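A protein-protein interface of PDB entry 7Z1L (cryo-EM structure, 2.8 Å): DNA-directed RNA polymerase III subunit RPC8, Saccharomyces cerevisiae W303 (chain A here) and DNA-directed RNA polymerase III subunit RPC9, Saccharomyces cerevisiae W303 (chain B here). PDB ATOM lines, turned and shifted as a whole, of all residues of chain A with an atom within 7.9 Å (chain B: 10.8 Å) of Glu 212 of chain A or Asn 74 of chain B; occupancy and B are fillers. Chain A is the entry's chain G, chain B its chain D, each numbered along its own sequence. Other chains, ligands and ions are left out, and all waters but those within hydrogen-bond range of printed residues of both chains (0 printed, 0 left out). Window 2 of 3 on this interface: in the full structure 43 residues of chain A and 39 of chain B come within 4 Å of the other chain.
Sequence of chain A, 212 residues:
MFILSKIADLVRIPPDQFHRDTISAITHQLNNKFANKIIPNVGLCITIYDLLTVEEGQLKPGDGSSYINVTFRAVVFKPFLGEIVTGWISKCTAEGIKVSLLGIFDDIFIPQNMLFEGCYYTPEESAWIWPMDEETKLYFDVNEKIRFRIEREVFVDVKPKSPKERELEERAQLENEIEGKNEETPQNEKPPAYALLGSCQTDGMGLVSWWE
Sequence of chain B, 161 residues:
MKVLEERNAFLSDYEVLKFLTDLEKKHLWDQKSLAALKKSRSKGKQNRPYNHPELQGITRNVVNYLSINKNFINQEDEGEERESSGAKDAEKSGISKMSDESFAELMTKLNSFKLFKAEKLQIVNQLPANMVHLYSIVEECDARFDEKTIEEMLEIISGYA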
ATOM      1  N   LYS A 145     -18.455 -26.764  19.071  1.00  0.00           N
ATOM      2  CA  LYS A 145     -17.161 -27.430  19.193  1.00  0.00           C
ATOM      3  C   LYS A 145     -16.212 -26.531  19.978  1.00  0.00           C
ATOM      4  O   LYS A 145     -15.533 -25.673  19.409  1.00  0.00           O
ATOM      5  CB  LYS A 145     -16.626 -27.752  17.803  1.00  0.00           C
ATOM      6  CG  LYS A 145     -17.418 -28.851  17.115  1.00  0.00           C
ATOM      7  CD  LYS A 145     -16.558 -29.703  16.214  1.00  0.00           C
ATOM      8  CE  LYS A 145     -16.843 -29.407  14.751  1.00  0.00           C
ATOM      9  NZ  LYS A 145     -16.456 -30.542  13.868  1.00  0.00           N
ATOM     10  N   LEU A 207     -14.090 -21.821  21.470  1.00  0.00           N
ATOM     11  CA  LEU A 207     -14.635 -22.389  20.246  1.00  0.00           C
ATOM     12  C   LEU A 207     -13.553 -22.532  19.181  1.00  0.00           C
ATOM     13  O   LEU A 207     -12.562 -21.798  19.157  1.00  0.00           O
ATOM     14  CB  LEU A 207     -15.773 -21.518  19.711  1.00  0.00           C
ATOM     15  CG  LEU A 207     -17.222 -21.787  20.130  1.00  0.00           C
ATOM     16  CD1 LEU A 207     -17.683 -23.128  19.597  1.00  0.00           C
ATOM     17  CD2 LEU A 207     -17.408 -21.708  21.643  1.00  0.00           C
ATOM     18  N   VAL A 208     -13.758 -23.503  18.289  1.00  0.00           N
ATOM     19  CA  VAL A 208     -12.817 -23.721  17.194  1.00  0.00           C
ATOM     20  C   VAL A 208     -12.927 -22.610  16.152  1.00  0.00           C
ATOM     21  O   VAL A 208     -11.925 -22.208  15.548  1.00  0.00           O
ATOM     22  CB  VAL A 208     -13.022 -25.122  16.581  1.00  0.00           C
ATOM     23  CG1 VAL A 208     -14.404 -25.268  15.951  1.00  0.00           C
ATOM     24  CG2 VAL A 208     -11.940 -25.419  15.554  1.00  0.00           C
ATOM     25  N   SER A 209     -14.134 -22.083  15.934  1.00  0.00           N
ATOM     26  CA  SER A 209     -14.329 -21.114  14.861  1.00  0.00           C
ATOM     27  C   SER A 209     -13.823 -19.728  15.240  1.00  0.00           C
ATOM     28  O   SER A 209     -13.548 -18.908  14.357  1.00  0.00           O
ATOM     29  CB  SER A 209     -15.808 -21.046  14.478  1.00  0.00           C
ATOM     30  OG  SER A 209     -16.602 -20.633  15.577  1.00  0.00           O
ATOM     31  N   TRP A 210     -13.695 -19.448  16.538  1.00  0.00           N
ATOM     32  CA  TRP A 210     -13.335 -18.102  16.975  1.00  0.00           C
ATOM     33  C   TRP A 210     -11.876 -17.790  16.670  1.00  0.00           C
ATOM     34  O   TRP A 210     -11.536 -16.656  16.315  1.00  0.00           O
ATOM     35  CB  TRP A 210     -13.629 -17.954  18.465  1.00  0.00           C
ATOM     36  CG  TRP A 210     -15.091 -17.957  18.797  1.00  0.00           C
ATOM     37  CD1 TRP A 210     -16.132 -18.170  17.937  1.00  0.00           C
ATOM     38  CD2 TRP A 210     -15.673 -17.777  20.090  1.00  0.00           C
ATOM     39  NE1 TRP A 210     -17.325 -18.109  18.614  1.00  0.00           N
ATOM     40  CE2 TRP A 210     -17.070 -17.872  19.939  1.00  0.00           C
ATOM     41  CE3 TRP A 210     -15.147 -17.537  21.362  1.00  0.00           C
ATOM     42  CZ2 TRP A 210     -17.946 -17.735  21.012  1.00  0.00           C
ATOM     43  CZ3 TRP A 210     -16.018 -17.401  22.423  1.00  0.00           C
ATOM     44  CH2 TRP A 210     -17.401 -17.502  22.243  1.00  0.00           C
ATOM     45  N   TRP A 211     -11.003 -18.783  16.802  1.00  0.00           N
ATOM     46  CA  TRP A 211      -9.592 -18.676  16.448  1.00  0.00           C
ATOM     47  C   TRP A 211      -9.292 -19.382  15.130  1.00  0.00           C
ATOM     48  O   TRP A 211      -8.253 -20.020  14.962  1.00  0.00           O
ATOM     49  CB  TRP A 211      -8.720 -19.198  17.584  1.00  0.00           C
ATOM     50  CG  TRP A 211      -8.778 -18.308  18.786  1.00  0.00           C
ATOM     51  CD1 TRP A 211      -7.965 -17.244  19.046  1.00  0.00           C
ATOM     52  CD2 TRP A 211      -9.738 -18.346  19.850  1.00  0.00           C
ATOM     53  NE1 TRP A 211      -8.328 -16.646  20.221  1.00  0.00           N
ATOM     54  CE2 TRP A 211      -9.417 -17.299  20.736  1.00  0.00           C
ATOM     55  CE3 TRP A 211     -10.818 -19.176  20.152  1.00  0.00           C
ATOM     56  CZ2 TRP A 211     -10.142 -17.058  21.895  1.00  0.00           C
ATOM     57  CZ3 TRP A 211     -11.539 -18.927  21.304  1.00  0.00           C
ATOM     58  CH2 TRP A 211     -11.193 -17.886  22.168  1.00  0.00           C
ATOM     59  N   GLU A 212     -10.222 -19.265  14.187  1.00  0.00           N
ATOM     60  CA  GLU A 212     -10.042 -19.771  12.834  1.00  0.00           C
ATOM     61  C   GLU A 212      -8.894 -19.051  12.131  1.00  0.00           C
ATOM     62  O   GLU A 212      -8.569 -17.911  12.464  1.00  0.00           O
ATOM     63  CB  GLU A 212     -11.333 -19.604  12.029  1.00  0.00           C
ATOM     64  CG  GLU A 212     -11.224 -20.037  10.583  1.00  0.00           C
ATOM     65  CD  GLU A 212     -12.530 -19.890   9.831  1.00  0.00           C
ATOM     66  OE1 GLU A 212     -13.528 -19.455  10.445  1.00  0.00           O
ATOM     67  OE2 GLU A 212     -12.557 -20.204   8.624  1.00  0.00           O
ATOM     68  N   ILE B  68     -13.810 -38.425  12.932  1.00  0.00           N
ATOM     69  CA  ILE B  68     -14.173 -37.083  12.498  1.00  0.00           C
ATOM     70  C   ILE B  68     -12.978 -36.162  12.683  1.00  0.00           C
ATOM     71  O   ILE B  68     -12.057 -36.455  13.457  1.00  0.00           O
ATOM     72  CB  ILE B  68     -15.403 -36.571  13.264  1.00  0.00           C
ATOM     73  CG1 ILE B  68     -15.101 -36.473  14.758  1.00  0.00           C
ATOM     74  CG2 ILE B  68     -16.600 -37.476  13.018  1.00  0.00           C
ATOM     75  CD1 ILE B  68     -16.176 -35.765  15.534  1.00  0.00           C
ATOM     76  N   ASN B  69     -12.992 -35.037  11.971  1.00  0.00           N
ATOM     77  CA  ASN B  69     -11.803 -34.204  11.860  1.00  0.00           C
ATOM     78  C   ASN B  69     -11.381 -33.592  13.193  1.00  0.00           C
ATOM     79  O   ASN B  69     -12.209 -33.258  14.044  1.00  0.00           O
ATOM     80  CB  ASN B  69     -12.008 -33.130  10.775  1.00  0.00           C
ATOM     81  CG  ASN B  69     -13.141 -32.143  11.080  1.00  0.00           C
ATOM     82  OD1 ASN B  69     -13.740 -32.139  12.152  1.00  0.00           O
ATOM     83  ND2 ASN B  69     -13.433 -31.290  10.104  1.00  0.00           N
ATOM     84  N   LYS B  70     -10.067 -33.526  13.400  1.00  0.00           N
ATOM     85  CA  LYS B  70      -9.527 -32.787  14.530  1.00  0.00           C
ATOM     86  C   LYS B  70      -9.830 -31.308  14.351  1.00  0.00           C
ATOM     87  O   LYS B  70      -9.765 -30.780  13.237  1.00  0.00           O
ATOM     88  CB  LYS B  70      -8.020 -33.019  14.651  1.00  0.00           C
ATOM     89  CG  LYS B  70      -7.561 -34.473  14.875  1.00  0.00           C
ATOM     90  CD  LYS B  70      -7.887 -35.031  16.271  1.00  0.00           C
ATOM     91  CE  LYS B  70      -9.206 -35.800  16.336  1.00  0.00           C
ATOM     92  NZ  LYS B  70      -9.426 -36.411  17.676  1.00  0.00           N
ATOM     93  N   ASN B  71     -10.173 -30.638  15.445  1.00  0.00           N
ATOM     94  CA  ASN B  71     -10.649 -29.259  15.362  1.00  0.00           C
ATOM     95  C   ASN B  71      -9.491 -28.266  15.465  1.00  0.00           C
ATOM     96  O   ASN B  71      -9.435 -27.395  16.332  1.00  0.00           O
ATOM     97  CB  ASN B  71     -11.715 -29.010  16.419  1.00  0.00           C
ATOM     98  CG  ASN B  71     -12.979 -29.788  16.139  1.00  0.00           C
ATOM     99  OD1 ASN B  71     -13.411 -30.615  16.941  1.00  0.00           O
ATOM    100  ND2 ASN B  71     -13.553 -29.561  14.965  1.00  0.00           N
ATOM    101  N   PHE B  72      -8.544 -28.431  14.543  1.00  0.00           N
ATOM    102  CA  PHE B  72      -7.604 -27.358  14.243  1.00  0.00           C
ATOM    103  C   PHE B  72      -8.283 -26.254  13.445  1.00  0.00           C
ATOM    104  O   PHE B  72      -7.862 -25.093  13.504  1.00  0.00           O
ATOM    105  CB  PHE B  72      -6.403 -27.917  13.477  1.00  0.00           C
ATOM    106  CG  PHE B  72      -6.774 -28.924  12.423  1.00  0.00           C
ATOM    107  CD1 PHE B  72      -7.240 -28.513  11.184  1.00  0.00           C
ATOM    108  CD2 PHE B  72      -6.664 -30.282  12.673  1.00  0.00           C
ATOM    109  CE1 PHE B  72      -7.590 -29.435  10.217  1.00  0.00           C
ATOM    110  CE2 PHE B  72      -7.009 -31.210  11.707  1.00  0.00           C
ATOM    111  CZ  PHE B  72      -7.477 -30.784  10.480  1.00  0.00           C
ATOM    112  N   ILE B  73      -9.329 -26.602  12.695  1.00  0.00           N
ATOM    113  CA  ILE B  73     -10.093 -25.660  11.889  1.00  0.00           C
ATOM    114  C   ILE B  73     -11.546 -26.115  11.911  1.00  0.00           C
ATOM    115  O   ILE B  73     -11.851 -27.264  12.251  1.00  0.00           O
ATOM    116  CB  ILE B  73      -9.545 -25.573  10.442  1.00  0.00           C
ATOM    117  CG1 ILE B  73      -9.908 -24.235   9.793  1.00  0.00           C
ATOM    118  CG2 ILE B  73     -10.051 -26.736   9.598  1.00  0.00           C
ATOM    119  CD1 ILE B  73      -9.145 -23.061  10.361  1.00  0.00           C
ATOM    120  N   ASN B  74     -12.451 -25.205  11.564  1.00  0.00           N
ATOM    121  CA  ASN B  74     -13.873 -25.529  11.535  1.00  0.00           C
ATOM    122  C   ASN B  74     -14.242 -26.467  10.382  1.00  0.00           C
ATOM    123  O   ASN B  74     -15.404 -26.836  10.217  1.00  0.00           O
ATOM    124  CB  ASN B  74     -14.709 -24.238  11.485  1.00  0.00           C
ATOM    125  CG  ASN B  74     -14.481 -23.412  10.219  1.00  0.00           C
ATOM    126  OD1 ASN B  74     -13.787 -23.823   9.287  1.00  0.00           O
ATOM    127  ND2 ASN B  74     -15.077 -22.226  10.189  1.00  0.00           N
ATOM    128  N   GLU B  91     -12.635 -33.046   6.245  1.00  0.00           N
ATOM    129  CA  GLU B  91     -13.588 -33.564   7.220  1.00  0.00           C
ATOM    130  C   GLU B  91     -13.056 -34.826   7.896  1.00  0.00           C
ATOM    131  O   GLU B  91     -13.789 -35.521   8.600  1.00  0.00           O
ATOM    132  CB  GLU B  91     -14.941 -33.847   6.558  1.00  0.00           C
ATOM    133  CG  GLU B  91     -14.945 -35.009   5.571  1.00  0.00           C
ATOM    134  CD  GLU B  91     -14.408 -34.628   4.205  1.00  0.00           C
ATOM    135  OE1 GLU B  91     -14.408 -33.422   3.879  1.00  0.00           O
ATOM    136  OE2 GLU B  91     -13.988 -35.534   3.456  1.00  0.00           O
ATOM    137  N   LYS B  92     -11.775 -35.112   7.682  1.00  0.00           N
ATOM    138  CA  LYS B  92     -11.108 -36.253   8.288  1.00  0.00           C
ATOM    139  C   LYS B  92     -10.037 -35.770   9.259  1.00  0.00           C
ATOM    140  O   LYS B  92      -9.516 -34.659   9.140  1.00  0.00           O
ATOM    141  CB  LYS B  92     -10.490 -37.167   7.223  1.00  0.00           C
ATOM    142  CG  LYS B  92     -11.512 -37.960   6.425  1.00  0.00           C
ATOM    143  CD  LYS B  92     -10.841 -38.964   5.502  1.00  0.00           C
ATOM    144  CE  LYS B  92     -10.206 -38.275   4.306  1.00  0.00           C
ATOM    145  NZ  LYS B  92     -11.227 -37.652   3.418  1.00  0.00           N
ATOM    146  N   LEU B 127      -2.700 -32.808  15.740  1.00  0.00           N
ATOM    147  CA  LEU B 127      -2.239 -32.256  14.462  1.00  0.00           C
ATOM    148  C   LEU B 127      -2.608 -30.784  14.327  1.00  0.00           C
ATOM    149  O   LEU B 127      -3.534 -30.450  13.577  1.00  0.00           O
ATOM    150  CB  LEU B 127      -2.808 -33.026  13.265  1.00  0.00           C
ATOM    151  CG  LEU B 127      -2.153 -34.313  12.748  1.00  0.00           C
ATOM    152  CD1 LEU B 127      -0.739 -34.041  12.247  1.00  0.00           C
ATOM    153  CD2 LEU B 127      -2.166 -35.425  13.769  1.00  0.00           C
ATOM    154  N   ALA B 129      -3.049 -27.120  13.123  1.00  0.00           N
ATOM    155  CA  ALA B 129      -2.925 -26.296  11.929  1.00  0.00           C
ATOM    156  C   ALA B 129      -3.091 -24.818  12.230  1.00  0.00           C
ATOM    157  O   ALA B 129      -2.507 -23.980  11.538  1.00  0.00           O
ATOM    158  CB  ALA B 129      -3.955 -26.723  10.873  1.00  0.00           C
ATOM    159  N   ASN B 130      -3.875 -24.480  13.249  1.00  0.00           N
ATOM    160  CA  ASN B 130      -3.989 -23.102  13.695  1.00  0.00           C
ATOM    161  C   ASN B 130      -2.694 -22.667  14.371  1.00  0.00           C
ATOM    162  O   ASN B 130      -1.976 -23.468  14.975  1.00  0.00           O
ATOM    163  CB  ASN B 130      -5.168 -22.955  14.661  1.00  0.00           C
ATOM    164  CG  ASN B 130      -5.479 -21.504  15.006  1.00  0.00           C
ATOM    165  OD1 ASN B 130      -4.807 -20.577  14.552  1.00  0.00           O
ATOM    166  ND2 ASN B 130      -6.504 -21.307  15.827  1.00  0.00           N
ATOM    167  N   MET B 131      -2.394 -21.374  14.247  1.00  0.00           N
ATOM    168  CA  MET B 131      -1.192 -20.824  14.864  1.00  0.00           C
ATOM    169  C   MET B 131      -1.356 -20.735  16.378  1.00  0.00           C
ATOM    170  O   MET B 131      -0.454 -21.113  17.140  1.00  0.00           O
ATOM    171  CB  MET B 131      -0.913 -19.446  14.263  1.00  0.00           C
ATOM    172  CG  MET B 131       0.393 -18.800  14.663  1.00  0.00           C
ATOM    173  SD  MET B 131       1.767 -19.758  14.000  1.00  0.00           S
ATOM    174  CE  MET B 131       3.079 -19.293  15.115  1.00  0.00           C
ATOM    175  N   VAL B 132      -2.518 -20.254  16.828  1.00  0.00           N
ATOM    176  CA  VAL B 132      -2.770 -20.065  18.251  1.00  0.00           C
ATOM    177  C   VAL B 132      -2.936 -21.406  18.960  1.00  0.00           C
ATOM    178  O   VAL B 132      -2.602 -21.536  20.141  1.00  0.00           O
ATOM    179  CB  VAL B 132      -4.000 -19.154  18.438  1.00  0.00           C
ATOM    180  CG1 VAL B 132      -4.178 -18.769  19.896  1.00  0.00           C
ATOM    181  CG2 VAL B 132      -3.872 -17.912  17.570  1.00  0.00           C
ATOM    182  N   HIS B 133      -3.448 -22.423  18.264  1.00  0.00           N
ATOM    183  CA  HIS B 133      -3.535 -23.753  18.862  1.00  0.00           C
ATOM    184  C   HIS B 133      -2.144 -24.327  19.122  1.00  0.00           C
ATOM    185  O   HIS B 133      -1.894 -24.935  20.175  1.00  0.00           O
ATOM    186  CB  HIS B 133      -4.356 -24.669  17.954  1.00  0.00           C
ATOM    187  CG  HIS B 133      -4.369 -26.104  18.378  1.00  0.00           C
ATOM    188  ND1 HIS B 133      -4.360 -27.144  17.475  1.00  0.00           N
ATOM    189  CD2 HIS B 133      -4.416 -26.673  19.606  1.00  0.00           C
ATOM    190  CE1 HIS B 133      -4.384 -28.293  18.127  1.00  0.00           C
ATOM    191  NE2 HIS B 133      -4.419 -28.035  19.422  1.00  0.00           N
ATOM    192  N   TYR B 160       0.962 -33.219   6.875  1.00  0.00           N
ATOM    193  CA  TYR B 160       0.426 -34.569   7.074  1.00  0.00           C
ATOM    194  C   TYR B 160       1.371 -35.634   6.515  1.00  0.00           C
ATOM    195  O   TYR B 160       1.043 -36.364   5.575  1.00  0.00           O
ATOM    196  CB  TYR B 160      -0.976 -34.701   6.472  1.00  0.00           C
ATOM    197  CG  TYR B 160      -2.005 -33.852   7.170  1.00  0.00           C
ATOM    198  CD1 TYR B 160      -1.974 -33.691   8.549  1.00  0.00           C
ATOM    199  CD2 TYR B 160      -3.002 -33.206   6.455  1.00  0.00           C
ATOM    200  CE1 TYR B 160      -2.909 -32.914   9.195  1.00  0.00           C
ATOM    201  CE2 TYR B 160      -3.942 -32.426   7.092  1.00  0.00           C
ATOM    202  CZ  TYR B 160      -3.890 -32.284   8.462  1.00  0.00           C
ATOM    203  OH  TYR B 160      -4.822 -31.508   9.101  1.00  0.00           O
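Of the 16 printed residues of chain B, 5 touch a printed residue of chain A. Along chain B the printed residues that touch a printed residue of chain A span positions 69 to 130. Printed residues of chain A that touch a printed residue of chain B: Lys 145, Val 208, Trp 211 and Glu 212.
The side-chain amide nitrogen (ND2) of Asn 71 of chain B lies close to the side-chain amino group (NZ) of Lys 145 of chain A. The side-chain amide nitrogen (ND2) of Asn 74 of chain B lies within hydrogen-bond range of the side-chain carboxylate (OE1) of Glu 212 of chain A (3.2 Å). O of Trp 211 of chain A sits close to ND2 of Asn 130 of chain B (2.3 Å).
Among the printed residues, merely in contact across the chains: Val 208 of chain A with Asn 71 of chain B (3.3 Å), Lys 145 of chain A with Asn 69 of chain B (3.6 Å), Glu 212 of chain A with Ile 73 of chain B (3.7 Å) and Val 208 of chain A with Ile 73 of chain B (3.7 Å).
Of the printed residues of chain B, Lys 145 of chain A touches Asn 69 and Asn 71. Leu 207 of chain A touches none of the printed residues of chain B. Glu 212 of chain A touches just these residues of chain B: Ile 73 (3.7 Å) and Asn 74 (3.2 Å). Of the printed residues of chain A, Asn 69 of chain B touches Lys 145 (3.6 Å). Printed residues of chain A within 4 Å of Asn 71 of chain B: Lys 145 (3.3 Å) and Val 208 (3.3 Å). Asn 74 of chain B touches just one residue of chain A: Glu 212 (3.2 Å). Glu 91 of chain B touches none of the printed residues of chain A. Printed residues of chain A within 4 Å of Asn 130 of chain B: Trp 211 (2.3 Å). The nearest residue of chain A that does not touch Asn 74 of chain B is Val 208 of chain A (4.03 Å). The nearest printed residue of chain A that does not touch Asn 71 of chain B is Leu 207 of chain A (7.0 Å).
The backbone NH (N) of Asn 69 of chain B is in hydrogen-bond range of the backbone carbonyl oxygen (O) of Glu 91 of chain B (3.5 Å). OD1 of Asn 130 of chain B is in hydrogen-bond range of N of Val 132 of chain B, at 3.2 Å. The backbone carbonyl oxygen (O) of Lys 145 of chain A is in hydrogen-bond range of the backbone NH (N) of Val 208 of chain A (3.0 Å).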
